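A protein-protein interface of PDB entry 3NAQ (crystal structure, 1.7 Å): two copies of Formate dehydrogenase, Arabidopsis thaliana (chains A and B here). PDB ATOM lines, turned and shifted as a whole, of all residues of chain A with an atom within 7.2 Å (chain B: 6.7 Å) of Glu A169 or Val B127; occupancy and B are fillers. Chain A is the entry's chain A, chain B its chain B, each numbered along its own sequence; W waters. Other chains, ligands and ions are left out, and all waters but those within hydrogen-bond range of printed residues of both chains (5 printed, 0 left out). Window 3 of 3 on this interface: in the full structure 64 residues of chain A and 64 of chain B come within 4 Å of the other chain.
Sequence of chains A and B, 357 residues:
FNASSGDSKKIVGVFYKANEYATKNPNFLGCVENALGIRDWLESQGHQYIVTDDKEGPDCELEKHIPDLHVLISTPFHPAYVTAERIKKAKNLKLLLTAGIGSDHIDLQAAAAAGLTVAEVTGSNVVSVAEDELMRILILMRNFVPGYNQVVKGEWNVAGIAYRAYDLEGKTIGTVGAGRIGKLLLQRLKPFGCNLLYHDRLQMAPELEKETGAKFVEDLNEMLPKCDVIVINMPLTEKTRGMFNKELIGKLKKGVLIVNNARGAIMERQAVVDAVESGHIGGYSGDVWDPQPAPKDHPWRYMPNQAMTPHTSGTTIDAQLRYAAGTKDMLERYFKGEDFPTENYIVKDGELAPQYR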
ATOM      1  N   LEU A 138      17.794 -34.271 -18.512  1.00  0.00           N
ATOM      2  CA  LEU A 138      17.230 -32.918 -18.530  1.00  0.00           C
ATOM      3  C   LEU A 138      16.378 -32.616 -17.314  1.00  0.00           C
ATOM      4  O   LEU A 138      16.495 -31.525 -16.743  1.00  0.00           O
ATOM      5  CB  LEU A 138      16.408 -32.765 -19.778  1.00  0.00           C
ATOM      6  CG  LEU A 138      17.201 -32.649 -21.065  1.00  0.00           C
ATOM      7  CD1 LEU A 138      16.301 -32.902 -22.282  1.00  0.00           C
ATOM      8  CD2 LEU A 138      17.844 -31.275 -21.123  1.00  0.00           C
ATOM      9  N   MET A 141      18.886 -32.060 -14.527  1.00  0.00           N
ATOM     10  CA  MET A 141      19.787 -30.925 -14.769  1.00  0.00           C
ATOM     11  C   MET A 141      19.018 -29.601 -14.659  1.00  0.00           C
ATOM     12  O   MET A 141      19.482 -28.654 -14.024  1.00  0.00           O
ATOM     13  CB  MET A 141      20.411 -31.014 -16.152  1.00  0.00           C
ATOM     14  CG  MET A 141      21.462 -29.949 -16.394  1.00  0.00           C
ATOM     15  SD  MET A 141      22.824 -29.948 -15.253  1.00  0.00           S
ATOM     16  CE  MET A 141      23.688 -31.497 -15.719  1.00  0.00           C
ATOM     17  N   ARG A 142      17.875 -29.576 -15.283  1.00  0.00           N
ATOM     18  CA  ARG A 142      17.042 -28.364 -15.381  1.00  0.00           C
ATOM     19  C   ARG A 142      16.072 -28.218 -14.219  1.00  0.00           C
ATOM     20  O   ARG A 142      15.347 -27.230 -14.132  1.00  0.00           O
ATOM     21  CB  ARG A 142      16.333 -28.340 -16.731  1.00  0.00           C
ATOM     22  CG  ARG A 142      17.246 -28.415 -17.914  1.00  0.00           C
ATOM     23  CD  ARG A 142      16.592 -28.071 -19.265  1.00  0.00           C
ATOM     24  NE  ARG A 142      16.001 -26.754 -19.157  1.00  0.00           N
ATOM     25  CZ  ARG A 142      16.672 -25.601 -19.204  1.00  0.00           C
ATOM     26  NH1 ARG A 142      17.944 -25.566 -19.536  1.00  0.00           N
ATOM     27  NH2 ARG A 142      16.038 -24.477 -18.920  1.00  0.00           N
ATOM     28  N   TYR A 166      20.217 -25.844 -14.085  1.00  0.00           N
ATOM     29  CA  TYR A 166      21.319 -25.575 -14.980  1.00  0.00           C
ATOM     30  C   TYR A 166      20.917 -25.952 -16.354  1.00  0.00           C
ATOM     31  O   TYR A 166      20.045 -26.767 -16.518  1.00  0.00           O
ATOM     32  CB  TYR A 166      22.500 -26.451 -14.587  1.00  0.00           C
ATOM     33  CG  TYR A 166      23.180 -25.963 -13.324  1.00  0.00           C
ATOM     34  CD1 TYR A 166      24.308 -25.203 -13.400  1.00  0.00           C
ATOM     35  CD2 TYR A 166      22.688 -26.274 -12.049  1.00  0.00           C
ATOM     36  CE1 TYR A 166      24.966 -24.731 -12.272  1.00  0.00           C
ATOM     37  CE2 TYR A 166      23.336 -25.793 -10.927  1.00  0.00           C
ATOM     38  CZ  TYR A 166      24.494 -25.054 -11.048  1.00  0.00           C
ATOM     39  OH  TYR A 166      25.204 -24.528  -9.971  1.00  0.00           O
ATOM     40  N   ASP A 167      21.639 -25.464 -17.345  1.00  0.00           N
ATOM     41  CA  ASP A 167      21.466 -25.946 -18.693  1.00  0.00           C
ATOM     42  C   ASP A 167      22.296 -27.187 -18.838  1.00  0.00           C
ATOM     43  O   ASP A 167      23.333 -27.341 -18.170  1.00  0.00           O
ATOM     44  CB  ASP A 167      21.969 -24.908 -19.704  1.00  0.00           C
ATOM     45  CG  ASP A 167      21.127 -23.664 -19.747  1.00  0.00           C
ATOM     46  OD1 ASP A 167      19.968 -23.607 -19.192  1.00  0.00           O
ATOM     47  OD2 ASP A 167      21.645 -22.713 -20.374  1.00  0.00           O
ATOM     48  N   LEU A 168      21.896 -28.061 -19.760  1.00  0.00           N
ATOM     49  CA  LEU A 168      22.676 -29.238 -20.037  1.00  0.00           C
ATOM     50  C   LEU A 168      23.927 -28.931 -20.840  1.00  0.00           C
ATOM     51  O   LEU A 168      24.951 -29.587 -20.726  1.00  0.00           O
ATOM     52  CB  LEU A 168      21.764 -30.264 -20.706  1.00  0.00           C
ATOM     53  CG  LEU A 168      22.371 -31.604 -21.073  1.00  0.00           C
ATOM     54  CD1 LEU A 168      22.944 -32.221 -19.835  1.00  0.00           C
ATOM     55  CD2 LEU A 168      21.347 -32.532 -21.787  1.00  0.00           C
ATOM     56  N   GLU A 169      23.828 -27.922 -21.677  1.00  0.00           N
ATOM     57  CA  GLU A 169      24.917 -27.439 -22.477  1.00  0.00           C
ATOM     58  C   GLU A 169      26.152 -27.274 -21.607  1.00  0.00           C
ATOM     59  O   GLU A 169      26.081 -26.720 -20.494  1.00  0.00           O
ATOM     60  CB  GLU A 169      24.548 -26.106 -23.125  1.00  0.00           C
ATOM     61  CG  GLU A 169      25.634 -25.587 -24.043  1.00  0.00           C
ATOM     62  CD  GLU A 169      25.362 -24.202 -24.620  1.00  0.00           C
ATOM     63  OE1 GLU A 169      24.786 -23.336 -23.911  1.00  0.00           O
ATOM     64  OE2 GLU A 169      25.699 -23.986 -25.815  1.00  0.00           O
ATOM     65  N   GLY A 170      27.273 -27.805 -22.089  1.00  0.00           N
ATOM     66  CA  GLY A 170      28.534 -27.576 -21.420  1.00  0.00           C
ATOM     67  C   GLY A 170      28.885 -28.554 -20.333  1.00  0.00           C
ATOM     68  O   GLY A 170      30.040 -28.598 -19.917  1.00  0.00           O
ATOM     69  N   LYS A 171      27.932 -29.383 -19.930  1.00  0.00           N
ATOM     70  CA  LYS A 171      28.104 -30.268 -18.804  1.00  0.00           C
ATOM     71  C   LYS A 171      28.800 -31.518 -19.254  1.00  0.00           C
ATOM     72  O   LYS A 171      28.753 -31.891 -20.436  1.00  0.00           O
ATOM     73  CB  LYS A 171      26.785 -30.626 -18.163  1.00  0.00           C
ATOM     74  CG  LYS A 171      25.943 -29.427 -17.724  1.00  0.00           C
ATOM     75  CD  LYS A 171      26.653 -28.603 -16.645  1.00  0.00           C
ATOM     76  CE  LYS A 171      25.918 -27.356 -16.280  1.00  0.00           C
ATOM     77  NZ  LYS A 171      25.810 -26.365 -17.456  1.00  0.00           N
ATOM     78  N   THR A 172      29.498 -32.144 -18.315  1.00  0.00           N
ATOM     79  CA  THR A 172      30.183 -33.410 -18.592  1.00  0.00           C
ATOM     80  C   THR A 172      29.228 -34.544 -18.244  1.00  0.00           C
ATOM     81  O   THR A 172      28.753 -34.638 -17.123  1.00  0.00           O
ATOM     82  CB  THR A 172      31.478 -33.556 -17.816  1.00  0.00           C
ATOM     83  OG1 THR A 172      32.381 -32.511 -18.206  1.00  0.00           O
ATOM     84  CG2 THR A 172      32.143 -34.925 -18.156  1.00  0.00           C
ATOM     85  N   PRO A 191      23.789 -33.062 -29.990  1.00  0.00           N
ATOM     86  CA  PRO A 191      23.484 -31.684 -30.315  1.00  0.00           C
ATOM     87  C   PRO A 191      23.364 -30.783 -29.141  1.00  0.00           C
ATOM     88  O   PRO A 191      23.281 -29.594 -29.352  1.00  0.00           O
ATOM     89  CB  PRO A 191      22.113 -31.757 -31.009  1.00  0.00           C
ATOM     90  CG  PRO A 191      21.555 -33.022 -30.658  1.00  0.00           C
ATOM     91  CD  PRO A 191      22.700 -33.961 -30.393  1.00  0.00           C
ATOM     92  N   PHE A 192      23.341 -31.324 -27.915  1.00  0.00           N
ATOM     93  CA  PHE A 192      23.229 -30.468 -26.758  1.00  0.00           C
ATOM     94  C   PHE A 192      24.519 -29.713 -26.407  1.00  0.00           C
ATOM     95  O   PHE A 192      24.486 -28.822 -25.562  1.00  0.00           O
ATOM     96  CB  PHE A 192      22.710 -31.222 -25.559  1.00  0.00           C
ATOM     97  CG  PHE A 192      21.259 -31.622 -25.677  1.00  0.00           C
ATOM     98  CD1 PHE A 192      20.895 -32.765 -26.355  1.00  0.00           C
ATOM     99  CD2 PHE A 192      20.270 -30.868 -25.090  1.00  0.00           C
ATOM    100  CE1 PHE A 192      19.564 -33.152 -26.443  1.00  0.00           C
ATOM    101  CE2 PHE A 192      18.940 -31.247 -25.191  1.00  0.00           C
ATOM    102  CZ  PHE A 192      18.582 -32.358 -25.831  1.00  0.00           C
ATOM    103  N   GLY A 193      25.640 -30.084 -27.016  1.00  0.00           N
ATOM    104  CA  GLY A 193      26.876 -29.364 -26.759  1.00  0.00           C
ATOM    105  C   GLY A 193      27.464 -29.626 -25.379  1.00  0.00           C
ATOM    106  O   GLY A 193      27.990 -28.708 -24.718  1.00  0.00           O
ATOM    107  N   CYS A 194      27.455 -30.906 -25.005  1.00  0.00           N
ATOM    108  CA  CYS A 194      28.030 -31.412 -23.752  1.00  0.00           C
ATOM    109  C   CYS A 194      29.415 -31.976 -24.005  1.00  0.00           C
ATOM    110  O   CYS A 194      29.849 -32.102 -25.143  1.00  0.00           O
ATOM    111  CB  CYS A 194      27.169 -32.529 -23.227  1.00  0.00           C
ATOM    112  SG  CYS A 194      25.436 -32.056 -23.056  1.00  0.00           S
ATOM    113  N   ASN A 195      30.102 -32.245 -22.912  1.00  0.00           N
ATOM    114  CA  ASN A 195      31.339 -32.990 -22.917  1.00  0.00           C
ATOM    115  C   ASN A 195      30.974 -34.432 -22.576  1.00  0.00           C
ATOM    116  O   ASN A 195      30.732 -34.771 -21.413  1.00  0.00           O
ATOM    117  CB  ASN A 195      32.286 -32.392 -21.878  1.00  0.00           C
ATOM    118  CG  ASN A 195      33.620 -33.104 -21.809  1.00  0.00           C
ATOM    119  OD1 ASN A 195      34.200 -33.215 -20.733  1.00  0.00           O
ATOM    120  ND2 ASN A 195      34.119 -33.586 -22.955  1.00  0.00           N
ATOM    121  N   GLY B 123      19.906 -12.626 -26.504  1.00  0.00           N
ATOM    122  CA  GLY B 123      20.277 -13.919 -27.047  1.00  0.00           C
ATOM    123  C   GLY B 123      20.786 -14.894 -26.047  1.00  0.00           C
ATOM    124  O   GLY B 123      21.137 -16.034 -26.418  1.00  0.00           O
ATOM    125  N   SER B 124      20.817 -14.470 -24.788  1.00  0.00           N
ATOM    126  CA  SER B 124      21.490 -15.207 -23.768  1.00  0.00           C
ATOM    127  C   SER B 124      20.625 -16.320 -23.132  1.00  0.00           C
ATOM    128  O   SER B 124      21.148 -17.112 -22.373  1.00  0.00           O
ATOM    129  CB  SER B 124      22.015 -14.273 -22.693  1.00  0.00           C
ATOM    130  OG  SER B 124      20.986 -13.375 -22.259  1.00  0.00           O
ATOM    131  N   ASN B 125      19.332 -16.370 -23.443  1.00  0.00           N
ATOM    132  CA  ASN B 125      18.439 -17.377 -22.908  1.00  0.00           C
ATOM    133  C   ASN B 125      18.095 -18.501 -23.891  1.00  0.00           C
ATOM    134  O   ASN B 125      17.337 -19.388 -23.541  1.00  0.00           O
ATOM    135  CB  ASN B 125      17.138 -16.778 -22.386  1.00  0.00           C
ATOM    136  CG  ASN B 125      16.285 -16.175 -23.484  1.00  0.00           C
ATOM    137  OD1 ASN B 125      16.804 -15.772 -24.531  1.00  0.00           O
ATOM    138  ND2 ASN B 125      14.970 -16.027 -23.226  1.00  0.00           N
ATOM    139  N   VAL B 126      18.593 -18.421 -25.136  1.00  0.00           N
ATOM    140  CA  VAL B 126      18.004 -19.197 -26.201  1.00  0.00           C
ATOM    141  C   VAL B 126      18.290 -20.688 -26.037  1.00  0.00           C
ATOM    142  O   VAL B 126      17.402 -21.510 -26.234  1.00  0.00           O
ATOM    143  CB  VAL B 126      18.400 -18.666 -27.628  1.00  0.00           C
ATOM    144  CG1 VAL B 126      17.807 -17.289 -27.831  1.00  0.00           C
ATOM    145  CG2 VAL B 126      19.900 -18.684 -27.818  1.00  0.00           C
ATOM    146  N   VAL B 127      19.498 -21.060 -25.624  1.00  0.00           N
ATOM    147  CA  VAL B 127      19.774 -22.499 -25.493  1.00  0.00           C
ATOM    148  C   VAL B 127      18.926 -23.040 -24.349  1.00  0.00           C
ATOM    149  O   VAL B 127      18.381 -24.154 -24.418  1.00  0.00           O
ATOM    150  CB  VAL B 127      21.288 -22.792 -25.301  1.00  0.00           C
ATOM    151  CG1 VAL B 127      21.555 -24.284 -24.921  1.00  0.00           C
ATOM    152  CG2 VAL B 127      22.054 -22.410 -26.557  1.00  0.00           C
ATOM    153  N   SER B 128      18.845 -22.263 -23.283  1.00  0.00           N
ATOM    154  CA  SER B 128      18.118 -22.656 -22.077  1.00  0.00           C
ATOM    155  C   SER B 128      16.676 -22.977 -22.407  1.00  0.00           C
ATOM    156  O   SER B 128      16.151 -23.995 -22.017  1.00  0.00           O
ATOM    157  CB  SER B 128      18.171 -21.552 -21.003  1.00  0.00           C
ATOM    158  OG  SER B 128      19.453 -20.942 -20.915  1.00  0.00           O
ATOM    159  N   VAL B 129      15.997 -22.076 -23.102  1.00  0.00           N
ATOM    160  CA  VAL B 129      14.614 -22.332 -23.457  1.00  0.00           C
ATOM    161  C   VAL B 129      14.470 -23.523 -24.430  1.00  0.00           C
ATOM    162  O   VAL B 129      13.560 -24.315 -24.303  1.00  0.00           O
ATOM    163  CB  VAL B 129      13.914 -21.038 -24.006  1.00  0.00           C
ATOM    164  CG1 VAL B 129      12.471 -21.330 -24.397  1.00  0.00           C
ATOM    165  CG2 VAL B 129      14.004 -19.869 -23.008  1.00  0.00           C
ATOM    166  N   ALA B 130      15.350 -23.649 -25.418  1.00  0.00           N
ATOM    167  CA  ALA B 130      15.277 -24.737 -26.363  1.00  0.00           C
ATOM    168  C   ALA B 130      15.411 -26.097 -25.643  1.00  0.00           C
ATOM    169  O   ALA B 130      14.669 -27.055 -25.892  1.00  0.00           O
ATOM    170  CB  ALA B 130      16.371 -24.592 -27.407  1.00  0.00           C
ATOM    171  N   GLU B 131      16.374 -26.184 -24.737  1.00  0.00           N
ATOM    172  CA  GLU B 131      16.504 -27.371 -23.925  1.00  0.00           C
ATOM    173  C   GLU B 131      15.258 -27.700 -23.153  1.00  0.00           C
ATOM    174  O   GLU B 131      14.834 -28.858 -23.042  1.00  0.00           O
ATOM    175  CB  GLU B 131      17.631 -27.220 -22.908  1.00  0.00           C
ATOM    176  CG  GLU B 131      18.999 -27.233 -23.482  1.00  0.00           C
ATOM    177  CD  GLU B 131      20.068 -27.184 -22.404  1.00  0.00           C
ATOM    178  OE1 GLU B 131      19.708 -27.223 -21.183  1.00  0.00           O
ATOM    179  OE2 GLU B 131      21.271 -27.170 -22.776  1.00  0.00           O
ATOM    180  N   ASP B 132      14.671 -26.668 -22.555  1.00  0.00           N
ATOM    181  CA  ASP B 132      13.549 -26.873 -21.687  1.00  0.00           C
ATOM    182  C   ASP B 132      12.355 -27.357 -22.511  1.00  0.00           C
ATOM    183  O   ASP B 132      11.584 -28.215 -22.055  1.00  0.00           O
ATOM    184  CB  ASP B 132      13.234 -25.576 -20.968  1.00  0.00           C
ATOM    185  CG  ASP B 132      12.596 -25.794 -19.660  1.00  0.00           C
ATOM    186  OD1 ASP B 132      13.280 -26.273 -18.745  1.00  0.00           O
ATOM    187  OD2 ASP B 132      11.417 -25.406 -19.562  1.00  0.00           O
ATOM    188  N   ILE B 181      15.380 -19.953 -30.944  1.00  0.00           N
ATOM    189  CA  ILE B 181      15.014 -21.042 -30.032  1.00  0.00           C
ATOM    190  C   ILE B 181      14.470 -22.222 -30.823  1.00  0.00           C
ATOM    191  O   ILE B 181      14.913 -23.344 -30.622  1.00  0.00           O
ATOM    192  CB  ILE B 181      13.995 -20.556 -28.995  1.00  0.00           C
ATOM    193  CG1 ILE B 181      14.649 -19.491 -28.099  1.00  0.00           C
ATOM    194  CG2 ILE B 181      13.422 -21.721 -28.240  1.00  0.00           C
ATOM    195  CD1 ILE B 181      13.648 -18.768 -27.176  1.00  0.00           C
ATOM    196  N   LEU B 184      17.364 -24.100 -32.490  1.00  0.00           N
ATOM    197  CA  LEU B 184      18.137 -24.897 -31.545  1.00  0.00           C
ATOM    198  C   LEU B 184      17.378 -26.140 -31.118  1.00  0.00           C
ATOM    199  O   LEU B 184      17.968 -27.186 -30.882  1.00  0.00           O
ATOM    200  CB  LEU B 184      18.481 -24.077 -30.314  1.00  0.00           C
ATOM    201  CG  LEU B 184      19.323 -22.846 -30.547  1.00  0.00           C
ATOM    202  CD1 LEU B 184      19.254 -21.858 -29.343  1.00  0.00           C
ATOM    203  CD2 LEU B 184      20.744 -23.253 -30.830  1.00  0.00           C
ATOM    204  N   ARG B 188      18.341 -30.108 -31.705  1.00  0.00           N
ATOM    205  CA  ARG B 188      18.359 -31.118 -30.649  1.00  0.00           C
ATOM    206  C   ARG B 188      17.378 -32.268 -30.930  1.00  0.00           C
ATOM    207  O   ARG B 188      17.562 -33.364 -30.428  1.00  0.00           O
ATOM    208  CB  ARG B 188      18.107 -30.467 -29.305  1.00  0.00           C
ATOM    209  CG  ARG B 188      19.342 -29.652 -28.851  1.00  0.00           C
ATOM    210  CD  ARG B 188      19.020 -28.515 -27.938  1.00  0.00           C
ATOM    211  NE  ARG B 188      20.225 -27.825 -27.546  1.00  0.00           N
ATOM    212  CZ  ARG B 188      20.934 -27.034 -28.331  1.00  0.00           C
ATOM    213  NH1 ARG B 188      20.570 -26.808 -29.596  1.00  0.00           N
ATOM    214  NH2 ARG B 188      22.032 -26.478 -27.864  1.00  0.00           N
ATOM    215  N   SER B 313      12.761 -21.296 -16.989  1.00  0.00           N
ATOM    216  CA  SER B 313      13.685 -21.901 -17.983  1.00  0.00           C
ATOM    217  C   SER B 313      14.827 -21.003 -18.412  1.00  0.00           C
ATOM    218  O   SER B 313      15.891 -21.488 -18.817  1.00  0.00           O
ATOM    219  CB  SER B 313      12.949 -22.377 -19.228  1.00  0.00           C
ATOM    220  OG  SER B 313      12.349 -21.291 -19.912  1.00  0.00           O
ATOM    221  N   ASP B 318      23.208 -21.177 -15.572  1.00  0.00           N
ATOM    222  CA  ASP B 318      24.023 -20.894 -16.750  1.00  0.00           C
ATOM    223  C   ASP B 318      23.554 -19.666 -17.512  1.00  0.00           C
ATOM    224  O   ASP B 318      24.380 -18.864 -18.003  1.00  0.00           O
ATOM    225  CB  ASP B 318      24.120 -22.085 -17.627  1.00  0.00           C
ATOM    226  CG  ASP B 318      24.813 -23.227 -16.934  1.00  0.00           C
ATOM    227  OD1 ASP B 318      24.172 -24.258 -16.788  1.00  0.00           O
ATOM    228  OD2 ASP B 318      26.008 -23.096 -16.558  1.00  0.00           O
ATOM    229  N   ARG B 322      25.429 -15.853 -17.931  1.00  0.00           N
ATOM    230  CA  ARG B 322      25.501 -15.101 -19.151  1.00  0.00           C
ATOM    231  C   ARG B 322      24.904 -13.701 -18.980  1.00  0.00           C
ATOM    232  O   ARG B 322      25.506 -12.740 -19.462  1.00  0.00           O
ATOM    233  CB  ARG B 322      24.779 -15.823 -20.280  1.00  0.00           C
ATOM    234  CG  ARG B 322      25.567 -16.945 -20.832  1.00  0.00           C
ATOM    235  CD  ARG B 322      24.914 -17.514 -22.074  1.00  0.00           C
ATOM    236  NE  ARG B 322      23.659 -18.186 -21.821  1.00  0.00           N
ATOM    237  CZ  ARG B 322      23.551 -19.481 -21.489  1.00  0.00           C
ATOM    238  NH1 ARG B 322      24.623 -20.221 -21.301  1.00  0.00           N
ATOM    239  NH2 ARG B 322      22.339 -20.013 -21.325  1.00  0.00           N
HETATM  240  O   HOH W   1      21.944 -27.710 -25.235  1.00  0.00           O
HETATM  241  O   HOH W   2      25.851 -24.148 -19.842  1.00  0.00           O
HETATM  242  O   HOH W   3      24.118 -22.958 -21.478  1.00  0.00           O
HETATM  243  O   HOH W   4      25.084 -27.421 -29.063  1.00  0.00           O
HETATM  244  O   HOH W   5      24.300 -20.759 -24.539  1.00  0.00           O
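NH2 of Arg B322 is in salt-bridge range of OD2 of Asp A167 (2.9 Å). OD1 of Asp B318 is in hydrogen-bond range of N of Asp A167 (2.9 Å). The guanidinium group of Arg A142 is in salt-bridge range of the side-chain carboxylate of Glu B131, at 2.9 Å. The backbone carbonyl oxygen (O) of Ser B313 sits at hydrogen-bond distance from the guanidinium group (NH2) of Arg A142 (3.0 Å). OD1 of Asp B318 is in salt-bridge range of NZ of Lys A171 (2.8 Å). N of Leu A168 sits at hydrogen-bond distance from OE1 of Glu B131, at 2.7 Å. OE2 of Glu B131 lies within hydrogen-bond range of N of Glu A169, 2.9 Å away. OG of Ser B128 is in hydrogen-bond range of OD2 of Asp A167, at 2.9 Å. The guanidinium group (NH2) of Arg A142 sits at hydrogen-bond distance from the backbone carbonyl oxygen (O) of Ser B128, at 3.1 Å. OD1 of Asp B132 is in salt-bridge range of NE of Arg A142.
CD1 of Tyr A166 touches OD1 of Asp B318, 3.5 Å away. Glu B131 touches Asp A167. Glu A169 touches Val B127 (OE1 to CG1, 3.5 Å). Arg B188 touches Pro A191. CE2 of Phe A192 touches CD of Arg B188 (3.9 Å).
The side-chain amino group (NZ) of Lys A171 lies within hydrogen-bond range of the backbone carbonyl oxygen (O) of Glu A169, 3.1 Å away. NH1 of Arg A142 is in salt-bridge range of OD1 of Asp A167 (2.8 Å). The backbone carbonyl oxygen (O) of Lys A171 sits at hydrogen-bond distance from the backbone NH (N) of Asn A195 (2.8 Å). The side-chain amino group (NZ) of Lys A171 lies within hydrogen-bond range of the backbone carbonyl oxygen (O) of Asp A167, 2.8 Å away. The backbone NH (N) of Tyr A166 sits at hydrogen-bond distance from the backbone carbonyl oxygen (O) of Met A141. The guanidinium group of Arg B188 sits at hydrogen-bond distance from the backbone carbonyl oxygen of Leu B184 (2.9 Å).
No position is printed for both chains.
Water W3 lies within hydrogen-bond range of OE1 of Glu A169 (2.6 Å), OD2 of Asp A167 (2.7 Å) and NH1 of Arg B322 (2.8 Å). Water W1 lies within hydrogen-bond range of OE2 of Glu B131, O of Phe A192 and NE of Arg B188. Water W2 lies within hydrogen-bond range of O of Glu A169, NZ of Lys A171 and OD2 of Asp B318. Water W5 bridges the side-chain carboxylate of Glu A169 (2.7 Å) and the guanidinium group of Arg B322 (3.3 Å). Water W4 lies within hydrogen-bond range of O of Pro A191 (2.8 Å), N of Gly A193 (3.4 Å) and NH2 of Arg B188 (3.4 Å).
Printed residues of chain B within 4 Å of Tyr A166: Asp B318. Glu A169 touches just these residues of chain B: Val B127 (3.5 Å) and Glu B131 (2.9 Å). Of chain A, only Glu A169 comes within 4 Å of Val B127. Val B129 touches none of the printed residues of chain A. Ile B181 touches none of the printed residues of chain A. Printed residues of chain A within 4 Å of Arg B188: Pro A191 and Phe A192. Printed residues of chain A within 4 Å of Asp B318: Tyr A166 (3.5 Å), Asp A167 (2.9 Å) and Lys A171 (2.8 Å). Of the printed residues of chain A, Arg B322 touches Asp A167. The nearest printed residue of chain A that does not touch Glu B131 is Phe A192 (4.2 Å).
Hydrophobic or aromatic side chains of chain A within 4 Å of the printed part of chain B: Tyr A166, Leu A168, Pro A191 and Phe A192. Among the printed residues, 15 pairs touch across the chains. Among the printed residues, Asp or Glu carboxylates within 4 Å of a Lys or Arg side-chain nitrogen of the other chain: Arg A142 with Glu B131 (2.9 Å), Arg A142 with Asp B132 (2.8 Å), Asp A167 with Arg B322 (2.9 Å) and Lys A171 with Asp B318 (2.8 Å).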
